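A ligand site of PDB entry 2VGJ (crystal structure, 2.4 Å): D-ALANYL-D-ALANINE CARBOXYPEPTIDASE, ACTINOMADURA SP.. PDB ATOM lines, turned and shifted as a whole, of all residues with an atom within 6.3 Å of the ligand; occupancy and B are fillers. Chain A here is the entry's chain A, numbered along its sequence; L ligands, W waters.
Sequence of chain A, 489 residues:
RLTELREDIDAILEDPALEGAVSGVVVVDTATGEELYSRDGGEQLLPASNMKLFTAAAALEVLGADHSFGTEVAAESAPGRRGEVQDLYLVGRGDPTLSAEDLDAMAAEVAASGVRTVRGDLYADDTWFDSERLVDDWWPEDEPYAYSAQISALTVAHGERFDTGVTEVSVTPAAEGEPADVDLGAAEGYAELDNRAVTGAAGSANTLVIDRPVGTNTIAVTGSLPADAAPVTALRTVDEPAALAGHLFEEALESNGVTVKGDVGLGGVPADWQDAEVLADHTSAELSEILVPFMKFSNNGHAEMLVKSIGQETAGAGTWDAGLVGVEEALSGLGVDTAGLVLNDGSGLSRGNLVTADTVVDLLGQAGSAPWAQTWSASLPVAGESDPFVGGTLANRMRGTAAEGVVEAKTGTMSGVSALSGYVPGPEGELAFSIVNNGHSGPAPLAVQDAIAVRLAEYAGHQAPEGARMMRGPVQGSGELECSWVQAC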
ATOM      1  N   PRO A  47     -19.634  10.512 -15.592  1.00  0.00           N
ATOM      2  CA  PRO A  47     -19.042   9.387 -16.300  1.00  0.00           C
ATOM      3  C   PRO A  47     -17.753   9.662 -17.143  1.00  0.00           C
ATOM      4  O   PRO A  47     -16.994   8.713 -17.400  1.00  0.00           O
ATOM      5  CB  PRO A  47     -20.162   9.005 -17.252  1.00  0.00           C
ATOM      6  CG  PRO A  47     -20.734  10.246 -17.593  1.00  0.00           C
ATOM      7  CD  PRO A  47     -20.831  10.969 -16.316  1.00  0.00           C
ATOM      8  N   ALA A  48     -17.540  10.920 -17.563  1.00  0.00           N
ATOM      9  CA  ALA A  48     -16.626  11.206 -18.680  1.00  0.00           C
ATOM     10  C   ALA A  48     -16.789  10.090 -19.738  1.00  0.00           C
ATOM     11  O   ALA A  48     -17.920   9.584 -19.908  1.00  0.00           O
ATOM     12  CB  ALA A  48     -15.159  11.382 -18.217  1.00  0.00           C
ATOM     13  N   SER A  49     -15.729   9.672 -20.420  1.00  0.00           N
ATOM     14  CA  SER A  49     -15.863   8.697 -21.514  1.00  0.00           C
ATOM     15  C   SER A  49     -16.437   7.309 -21.173  1.00  0.00           C
ATOM     16  O   SER A  49     -16.688   6.505 -22.076  1.00  0.00           O
ATOM     17  CB  SER A  49     -14.554   8.573 -22.306  1.00  0.00           C
ATOM     18  OG  SER A  49     -14.188   9.828 -22.894  1.00  0.00           O
ATOM     19  N   ASN A  50     -16.703   7.035 -19.892  1.00  0.00           N
ATOM     20  CA  ASN A  50     -17.394   5.775 -19.551  1.00  0.00           C
ATOM     21  C   ASN A  50     -18.814   5.627 -20.113  1.00  0.00           C
ATOM     22  O   ASN A  50     -19.381   4.507 -20.180  1.00  0.00           O
ATOM     23  CB  ASN A  50     -17.348   5.482 -18.047  1.00  0.00           C
ATOM     24  CG  ASN A  50     -16.225   4.518 -17.670  1.00  0.00           C
ATOM     25  OD1 ASN A  50     -15.083   4.631 -18.149  1.00  0.00           O
ATOM     26  ND2 ASN A  50     -16.541   3.574 -16.806  1.00  0.00           N
ATOM     27  N   LYS A  52     -19.553   6.123 -23.266  1.00  0.00           N
ATOM     28  CA  LYS A  52     -19.437   5.369 -24.482  1.00  0.00           C
ATOM     29  C   LYS A  52     -19.816   3.881 -24.256  1.00  0.00           C
ATOM     30  O   LYS A  52     -20.274   3.192 -25.180  1.00  0.00           O
ATOM     31  CB  LYS A  52     -18.027   5.494 -25.020  1.00  0.00           C
ATOM     32  CG  LYS A  52     -17.769   6.813 -25.790  1.00  0.00           C
ATOM     33  CD  LYS A  52     -16.287   7.102 -26.008  1.00  0.00           C
ATOM     34  CE  LYS A  52     -16.121   8.515 -26.477  1.00  0.00           C
ATOM     35  NZ  LYS A  52     -14.970   9.258 -25.879  1.00  0.00           N
ATOM     36  N   TRP A 139     -17.868  23.355 -23.490  1.00  0.00           N
ATOM     37  CA  TRP A 139     -17.206  24.586 -23.128  1.00  0.00           C
ATOM     38  C   TRP A 139     -16.575  25.235 -24.367  1.00  0.00           C
ATOM     39  O   TRP A 139     -15.867  24.567 -25.107  1.00  0.00           O
ATOM     40  CB  TRP A 139     -16.116  24.270 -22.100  1.00  0.00           C
ATOM     41  CG  TRP A 139     -16.634  23.932 -20.734  1.00  0.00           C
ATOM     42  CD1 TRP A 139     -17.925  23.658 -20.410  1.00  0.00           C
ATOM     43  CD2 TRP A 139     -15.864  23.801 -19.529  1.00  0.00           C
ATOM     44  NE1 TRP A 139     -18.018  23.387 -19.074  1.00  0.00           N
ATOM     45  CE2 TRP A 139     -16.777  23.454 -18.498  1.00  0.00           C
ATOM     46  CE3 TRP A 139     -14.503  23.956 -19.198  1.00  0.00           C
ATOM     47  CZ2 TRP A 139     -16.370  23.266 -17.155  1.00  0.00           C
ATOM     48  CZ3 TRP A 139     -14.098  23.753 -17.879  1.00  0.00           C
ATOM     49  CH2 TRP A 139     -15.034  23.443 -16.864  1.00  0.00           C
ATOM     50  N   ASP A 142     -12.652  24.915 -25.218  1.00  0.00           N
ATOM     51  CA  ASP A 142     -12.288  23.570 -25.696  1.00  0.00           C
ATOM     52  C   ASP A 142     -12.396  23.308 -27.200  1.00  0.00           C
ATOM     53  O   ASP A 142     -11.948  22.263 -27.680  1.00  0.00           O
ATOM     54  CB  ASP A 142     -13.223  22.551 -25.068  1.00  0.00           C
ATOM     55  CG  ASP A 142     -12.916  22.295 -23.664  1.00  0.00           C
ATOM     56  OD1 ASP A 142     -11.803  22.654 -23.250  1.00  0.00           O
ATOM     57  OD2 ASP A 142     -13.758  21.703 -22.977  1.00  0.00           O
ATOM     58  N   TYR A 147     -11.035  16.240 -29.632  1.00  0.00           N
ATOM     59  CA  TYR A 147     -12.165  15.669 -28.890  1.00  0.00           C
ATOM     60  C   TYR A 147     -13.426  16.516 -28.908  1.00  0.00           C
ATOM     61  O   TYR A 147     -14.526  15.998 -28.630  1.00  0.00           O
ATOM     62  CB  TYR A 147     -11.771  15.353 -27.443  1.00  0.00           C
ATOM     63  CG  TYR A 147     -11.436  16.577 -26.588  1.00  0.00           C
ATOM     64  CD1 TYR A 147     -12.452  17.333 -26.007  1.00  0.00           C
ATOM     65  CD2 TYR A 147     -10.102  16.955 -26.345  1.00  0.00           C
ATOM     66  CE1 TYR A 147     -12.177  18.456 -25.225  1.00  0.00           C
ATOM     67  CE2 TYR A 147      -9.811  18.051 -25.572  1.00  0.00           C
ATOM     68  CZ  TYR A 147     -10.854  18.808 -25.007  1.00  0.00           C
ATOM     69  OH  TYR A 147     -10.586  19.894 -24.208  1.00  0.00           O
ATOM     70  N   SER A 148     -13.282  17.806 -29.251  1.00  0.00           N
ATOM     71  CA  SER A 148     -14.434  18.710 -29.323  1.00  0.00           C
ATOM     72  C   SER A 148     -14.845  19.155 -30.726  1.00  0.00           C
ATOM     73  O   SER A 148     -15.474  20.214 -30.935  1.00  0.00           O
ATOM     74  CB  SER A 148     -14.157  19.929 -28.494  1.00  0.00           C
ATOM     75  OG  SER A 148     -15.361  20.676 -28.415  1.00  0.00           O
ATOM     76  N   PHE A 297      -9.435   4.179 -28.583  1.00  0.00           N
ATOM     77  CA  PHE A 297      -8.883   5.522 -28.484  1.00  0.00           C
ATOM     78  C   PHE A 297      -9.866   6.529 -27.928  1.00  0.00           C
ATOM     79  O   PHE A 297      -9.555   7.707 -27.789  1.00  0.00           O
ATOM     80  CB  PHE A 297      -8.308   5.952 -29.829  1.00  0.00           C
ATOM     81  CG  PHE A 297      -7.297   4.987 -30.381  1.00  0.00           C
ATOM     82  CD1 PHE A 297      -6.175   4.659 -29.628  1.00  0.00           C
ATOM     83  CD2 PHE A 297      -7.454   4.413 -31.639  1.00  0.00           C
ATOM     84  CE1 PHE A 297      -5.236   3.761 -30.109  1.00  0.00           C
ATOM     85  CE2 PHE A 297      -6.509   3.522 -32.143  1.00  0.00           C
ATOM     86  CZ  PHE A 297      -5.399   3.193 -31.363  1.00  0.00           C
ATOM     87  N   SER A 298     -11.075   6.070 -27.597  1.00  0.00           N
ATOM     88  CA  SER A 298     -12.119   6.956 -27.050  1.00  0.00           C
ATOM     89  C   SER A 298     -12.469   8.155 -27.982  1.00  0.00           C
ATOM     90  O   SER A 298     -12.451   9.311 -27.555  1.00  0.00           O
ATOM     91  CB  SER A 298     -11.689   7.433 -25.667  1.00  0.00           C
ATOM     92  OG  SER A 298     -12.793   7.488 -24.791  1.00  0.00           O
ATOM     93  N   ASN A 299     -12.792   7.857 -29.245  1.00  0.00           N
ATOM     94  CA  ASN A 299     -13.159   8.892 -30.219  1.00  0.00           C
ATOM     95  C   ASN A 299     -14.557   9.518 -29.970  1.00  0.00           C
ATOM     96  O   ASN A 299     -15.548   8.804 -30.129  1.00  0.00           O
ATOM     97  CB  ASN A 299     -13.089   8.303 -31.618  1.00  0.00           C
ATOM     98  CG  ASN A 299     -13.053   9.367 -32.706  1.00  0.00           C
ATOM     99  OD1 ASN A 299     -12.463   9.146 -33.770  1.00  0.00           O
ATOM    100  ND2 ASN A 299     -13.682  10.494 -32.483  1.00  0.00           N
ATOM    101  N   ASN A 300     -14.604  10.831 -29.618  1.00  0.00           N
ATOM    102  CA  ASN A 300     -15.871  11.526 -29.244  1.00  0.00           C
ATOM    103  C   ASN A 300     -16.829  11.712 -30.432  1.00  0.00           C
ATOM    104  O   ASN A 300     -18.024  11.391 -30.339  1.00  0.00           O
ATOM    105  CB  ASN A 300     -15.588  12.938 -28.673  1.00  0.00           C
ATOM    106  CG  ASN A 300     -15.060  12.961 -27.231  1.00  0.00           C
ATOM    107  OD1 ASN A 300     -14.818  11.930 -26.609  1.00  0.00           O
ATOM    108  ND2 ASN A 300     -14.866  14.172 -26.707  1.00  0.00           N
ATOM    109  N   SER A 347     -20.647  10.710 -26.023  1.00  0.00           N
ATOM    110  CA  SER A 347     -19.191  10.604 -25.840  1.00  0.00           C
ATOM    111  C   SER A 347     -18.730  10.729 -24.386  1.00  0.00           C
ATOM    112  O   SER A 347     -17.684  10.176 -24.005  1.00  0.00           O
ATOM    113  CB  SER A 347     -18.465  11.643 -26.682  1.00  0.00           C
ATOM    114  OG  SER A 347     -18.756  12.972 -26.273  1.00  0.00           O
ATOM    115  N   GLY A 348     -19.488  11.440 -23.578  1.00  0.00           N
ATOM    116  CA  GLY A 348     -19.042  11.702 -22.214  1.00  0.00           C
ATOM    117  C   GLY A 348     -18.428  13.084 -22.001  1.00  0.00           C
ATOM    118  O   GLY A 348     -18.225  13.446 -20.851  1.00  0.00           O
ATOM    119  N   LEU A 349     -18.165  13.835 -23.081  1.00  0.00           N
ATOM    120  CA  LEU A 349     -17.676  15.214 -22.986  1.00  0.00           C
ATOM    121  C   LEU A 349     -18.553  16.121 -22.063  1.00  0.00           C
ATOM    122  O   LEU A 349     -18.051  16.944 -21.291  1.00  0.00           O
ATOM    123  CB  LEU A 349     -17.553  15.844 -24.385  1.00  0.00           C
ATOM    124  CG  LEU A 349     -16.422  16.845 -24.673  1.00  0.00           C
ATOM    125  CD1 LEU A 349     -16.585  17.713 -26.001  1.00  0.00           C
ATOM    126  CD2 LEU A 349     -16.134  17.746 -23.514  1.00  0.00           C
ATOM    127  N   ARG A 351     -20.858  17.664 -19.185  1.00  0.00           N
ATOM    128  CA  ARG A 351     -21.024  17.570 -17.732  1.00  0.00           C
ATOM    129  C   ARG A 351     -22.506  17.506 -17.282  1.00  0.00           C
ATOM    130  O   ARG A 351     -22.818  17.732 -16.110  1.00  0.00           O
ATOM    131  CB  ARG A 351     -20.331  18.761 -17.073  1.00  0.00           C
ATOM    132  CG  ARG A 351     -18.851  18.829 -17.407  1.00  0.00           C
ATOM    133  CD  ARG A 351     -18.062  19.543 -16.333  1.00  0.00           C
ATOM    134  NE  ARG A 351     -16.650  19.581 -16.677  1.00  0.00           N
ATOM    135  CZ  ARG A 351     -15.673  19.145 -15.894  1.00  0.00           C
ATOM    136  NH1 ARG A 351     -14.420  19.198 -16.298  1.00  0.00           N
ATOM    137  NH2 ARG A 351     -15.960  18.654 -14.696  1.00  0.00           N
ATOM    138  N   THR A 393      -6.149   3.175 -24.790  1.00  0.00           N
ATOM    139  CA  THR A 393      -5.800   4.165 -23.744  1.00  0.00           C
ATOM    140  C   THR A 393      -5.257   3.498 -22.447  1.00  0.00           C
ATOM    141  O   THR A 393      -5.057   4.144 -21.410  1.00  0.00           O
ATOM    142  CB  THR A 393      -6.985   5.078 -23.394  1.00  0.00           C
ATOM    143  OG1 THR A 393      -8.061   4.278 -22.894  1.00  0.00           O
ATOM    144  CG2 THR A 393      -7.446   5.909 -24.627  1.00  0.00           C
ATOM    145  N   LYS A 410     -12.918   0.289 -20.119  1.00  0.00           N
ATOM    146  CA  LYS A 410     -13.029   1.608 -20.747  1.00  0.00           C
ATOM    147  C   LYS A 410     -12.585   2.680 -19.745  1.00  0.00           C
ATOM    148  O   LYS A 410     -12.812   2.564 -18.529  1.00  0.00           O
ATOM    149  CB  LYS A 410     -14.469   1.850 -21.226  1.00  0.00           C
ATOM    150  CG  LYS A 410     -14.749   3.133 -22.049  1.00  0.00           C
ATOM    151  CD  LYS A 410     -14.040   3.084 -23.423  1.00  0.00           C
ATOM    152  CE  LYS A 410     -14.052   4.435 -24.129  1.00  0.00           C
ATOM    153  NZ  LYS A 410     -13.054   5.362 -23.567  1.00  0.00           N
ATOM    154  N   THR A 411     -11.943   3.728 -20.273  1.00  0.00           N
ATOM    155  CA  THR A 411     -11.413   4.833 -19.469  1.00  0.00           C
ATOM    156  C   THR A 411     -12.261   6.108 -19.654  1.00  0.00           C
ATOM    157  O   THR A 411     -13.384   6.041 -20.118  1.00  0.00           O
ATOM    158  CB  THR A 411      -9.898   5.088 -19.828  1.00  0.00           C
ATOM    159  OG1 THR A 411      -9.743   5.436 -21.203  1.00  0.00           O
ATOM    160  CG2 THR A 411      -9.047   3.868 -19.544  1.00  0.00           C
ATOM    161  N   GLY A 412     -11.717   7.264 -19.269  1.00  0.00           N
ATOM    162  CA  GLY A 412     -12.423   8.535 -19.409  1.00  0.00           C
ATOM    163  C   GLY A 412     -11.983   9.494 -18.331  1.00  0.00           C
ATOM    164  O   GLY A 412     -12.200   9.234 -17.148  1.00  0.00           O
ATOM    165  N   THR A 413     -11.366  10.613 -18.735  1.00  0.00           N
ATOM    166  CA  THR A 413     -10.875  11.613 -17.807  1.00  0.00           C
ATOM    167  C   THR A 413     -11.141  13.079 -18.284  1.00  0.00           C
ATOM    168  O   THR A 413     -10.971  13.380 -19.475  1.00  0.00           O
ATOM    169  CB  THR A 413      -9.340  11.341 -17.517  1.00  0.00           C
ATOM    170  OG1 THR A 413      -9.211  10.163 -16.713  1.00  0.00           O
ATOM    171  CG2 THR A 413      -8.660  12.488 -16.819  1.00  0.00           C
ATOM    172  N   MET A 414     -11.569  13.944 -17.345  1.00  0.00           N
ATOM    173  CA  MET A 414     -11.720  15.418 -17.477  1.00  0.00           C
ATOM    174  C   MET A 414     -11.134  16.039 -16.217  1.00  0.00           C
ATOM    175  O   MET A 414     -10.700  15.305 -15.328  1.00  0.00           O
ATOM    176  CB  MET A 414     -13.197  15.825 -17.426  1.00  0.00           C
ATOM    177  CG  MET A 414     -14.045  15.358 -18.517  1.00  0.00           C
ATOM    178  SD  MET A 414     -15.525  16.312 -18.499  1.00  0.00           S
ATOM    179  CE  MET A 414     -16.743  14.992 -18.332  1.00  0.00           C
ATOM    180  N   SER A 415     -11.186  17.364 -16.094  1.00  0.00           N
ATOM    181  CA  SER A 415     -10.925  18.046 -14.837  1.00  0.00           C
ATOM    182  C   SER A 415     -11.982  17.697 -13.805  1.00  0.00           C
ATOM    183  O   SER A 415     -13.165  18.071 -13.972  1.00  0.00           O
ATOM    184  CB  SER A 415     -10.942  19.540 -15.025  1.00  0.00           C
ATOM    185  OG  SER A 415      -9.752  19.902 -15.674  1.00  0.00           O
ATOM    186  N   GLY A 416     -11.530  16.964 -12.791  1.00  0.00           N
ATOM    187  CA  GLY A 416     -12.341  16.586 -11.610  1.00  0.00           C
ATOM    188  C   GLY A 416     -13.071  15.265 -11.678  1.00  0.00           C
ATOM    189  O   GLY A 416     -13.764  14.889 -10.719  1.00  0.00           O
HETATM  190  O1  LIG L   1      -8.323   8.658 -21.911  1.00  0.00           O
HETATM  191  C1  LIG L   1      -9.461   8.790 -22.396  1.00  0.00           C
HETATM  192  O2  LIG L   1     -10.360   7.922 -22.161  1.00  0.00           O
HETATM  193  C2  LIG L   1      -9.744   9.963 -23.230  1.00  0.00           C
HETATM  194  N1  LIG L   1     -10.996  10.237 -23.360  1.00  0.00           N
HETATM  195  C3  LIG L   1      -8.722  10.812 -23.862  1.00  0.00           C
HETATM  196  C4  LIG L   1      -7.428  10.429 -23.994  1.00  0.00           C
HETATM  197  C5  LIG L   1      -9.129  12.196 -24.377  1.00  0.00           C
HETATM  198  S1  LIG L   1     -10.679  12.132 -25.234  1.00  0.00           S
HETATM  199  C6  LIG L   1     -11.738  11.048 -24.332  1.00  0.00           C
HETATM  200  C7  LIG L   1     -12.822  11.812 -23.539  1.00  0.00           C
HETATM  201  C8  LIG L   1     -13.432  10.899 -22.499  1.00  0.00           C
HETATM  202  O3  LIG L   1     -13.333  11.082 -21.300  1.00  0.00           O
HETATM  203  N2  LIG L   1     -12.227  12.914 -22.772  1.00  0.00           N
HETATM  204  C9  LIG L   1     -12.399  14.230 -22.959  1.00  0.00           C
HETATM  205  O4  LIG L   1     -13.047  14.768 -23.856  1.00  0.00           O
HETATM  206  C10 LIG L   1     -11.653  15.077 -21.962  1.00  0.00           C
HETATM  207  C11 LIG L   1     -12.465  16.289 -21.545  1.00  0.00           C
HETATM  208  C12 LIG L   1     -11.615  17.557 -21.441  1.00  0.00           C
HETATM  209  C13 LIG L   1     -12.582  18.715 -21.200  1.00  0.00           C
HETATM  210  C14 LIG L   1     -12.054  19.969 -20.461  1.00  0.00           C
HETATM  211  N3  LIG L   1     -13.023  21.067 -20.623  1.00  0.00           N
HETATM  212  C15 LIG L   1     -11.884  19.758 -19.003  1.00  0.00           C
HETATM  213  O5  LIG L   1     -12.804  20.077 -18.264  1.00  0.00           O
HETATM  214  O6  LIG L   1     -10.837  19.303 -18.518  1.00  0.00           O
HETATM  215  O   HOH W   1      -7.152   7.923 -19.817  1.00  0.00           O
HETATM  216  O   HOH W   2     -15.813  19.826 -19.950  1.00  0.00           O
HETATM  217  O   HOH W   3      -6.902   9.379 -26.681  1.00  0.00           O
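The backbone NH of Ser 49 lies within hydrogen-bond range of an oxygen (O3) of the ligand (2.9 Å). OG of Ser 49 is bonded to C8 of the ligand. OD2 of Asp 142 is in salt-bridge range of N3 of the ligand. The guanidinium group of Arg 351 is in salt-bridge range of an oxygen (O5) of the ligand, at 2.7 Å. O2 of the ligand sits at hydrogen-bond distance from OG1 of Thr 411 (2.7 Å). N of Thr 413 is in hydrogen-bond range of O3 of the ligand. N of Ser 415 sits at hydrogen-bond distance from O6 of the ligand (3.1 Å). An oxygen (O6) of the ligand lies within hydrogen-bond range of the side-chain hydroxyl (OG) of Ser 415 (3.1 Å). The backbone NH of Gly 412 is in hydrogen-bond range of an oxygen (O2) of the ligand (3.3 Å). An oxygen (O4) of the ligand is in hydrogen-bond range of the side-chain amide nitrogen (ND2) of Asn 300. O2 of the ligand is in salt-bridge range of NZ of Lys 410 (3.97 Å).
The side-chain hydroxyl of Ser 49 sits close to the side-chain hydroxyl of Ser 298 (3.3 Å). The side-chain hydroxyl (OG) of Ser 49 sits at hydrogen-bond distance from the side-chain amino group (NZ) of Lys 52 (3.1 Å). The guanidinium group (NH1) of Arg 351 sits close to the side-chain sulfur (SD) of Met 414 (3.8 Å). OG1 of Thr 411 sits at hydrogen-bond distance from OG1 of Thr 393 (2.7 Å). O of Tyr 147 is in hydrogen-bond range of ND2 of Asn 300 (2.7 Å). The side-chain amino group (NZ) of Lys 52 is in hydrogen-bond range of the side-chain amide oxygen (OD1) of Asn 300 (2.8 Å). The side-chain hydroxyl (OG) of Ser 298 is in hydrogen-bond range of the side-chain amino group (NZ) of Lys 410, at 2.5 Å. The side-chain amino group (NZ) of Lys 52 lies within hydrogen-bond range of the side-chain hydroxyl (OG) of Ser 298 (3.0 Å).
Residues that only touch the ligand: Tyr 147 (3.4 Å), Met 414 (3.5 Å), Trp 139 (3.5 Å), Ser 298 (3.6 Å), Ala 48 (3.6 Å) and Thr 393 (3.96 Å). Hydrophobic or aromatic side chains within 4 Å of the ligand: Ala 48, Trp 139, Tyr 147 and Met 414. 15 residues have an atom within 4 Å of the ligand: Ala 48, Ser 49, Trp 139, Asp 142, Tyr 147, Ser 298, Asn 300, Arg 351, Thr 393, Lys 410, Thr 411, Gly 412, Thr 413, Met 414 and Ser 415. The nearest printed residue that does not touch the ligand is Lys 52 (4.01 Å).
Water W2 lies within hydrogen-bond range of N3 of the ligand (3.1 Å) and NE of Arg 351 (3.4 Å).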
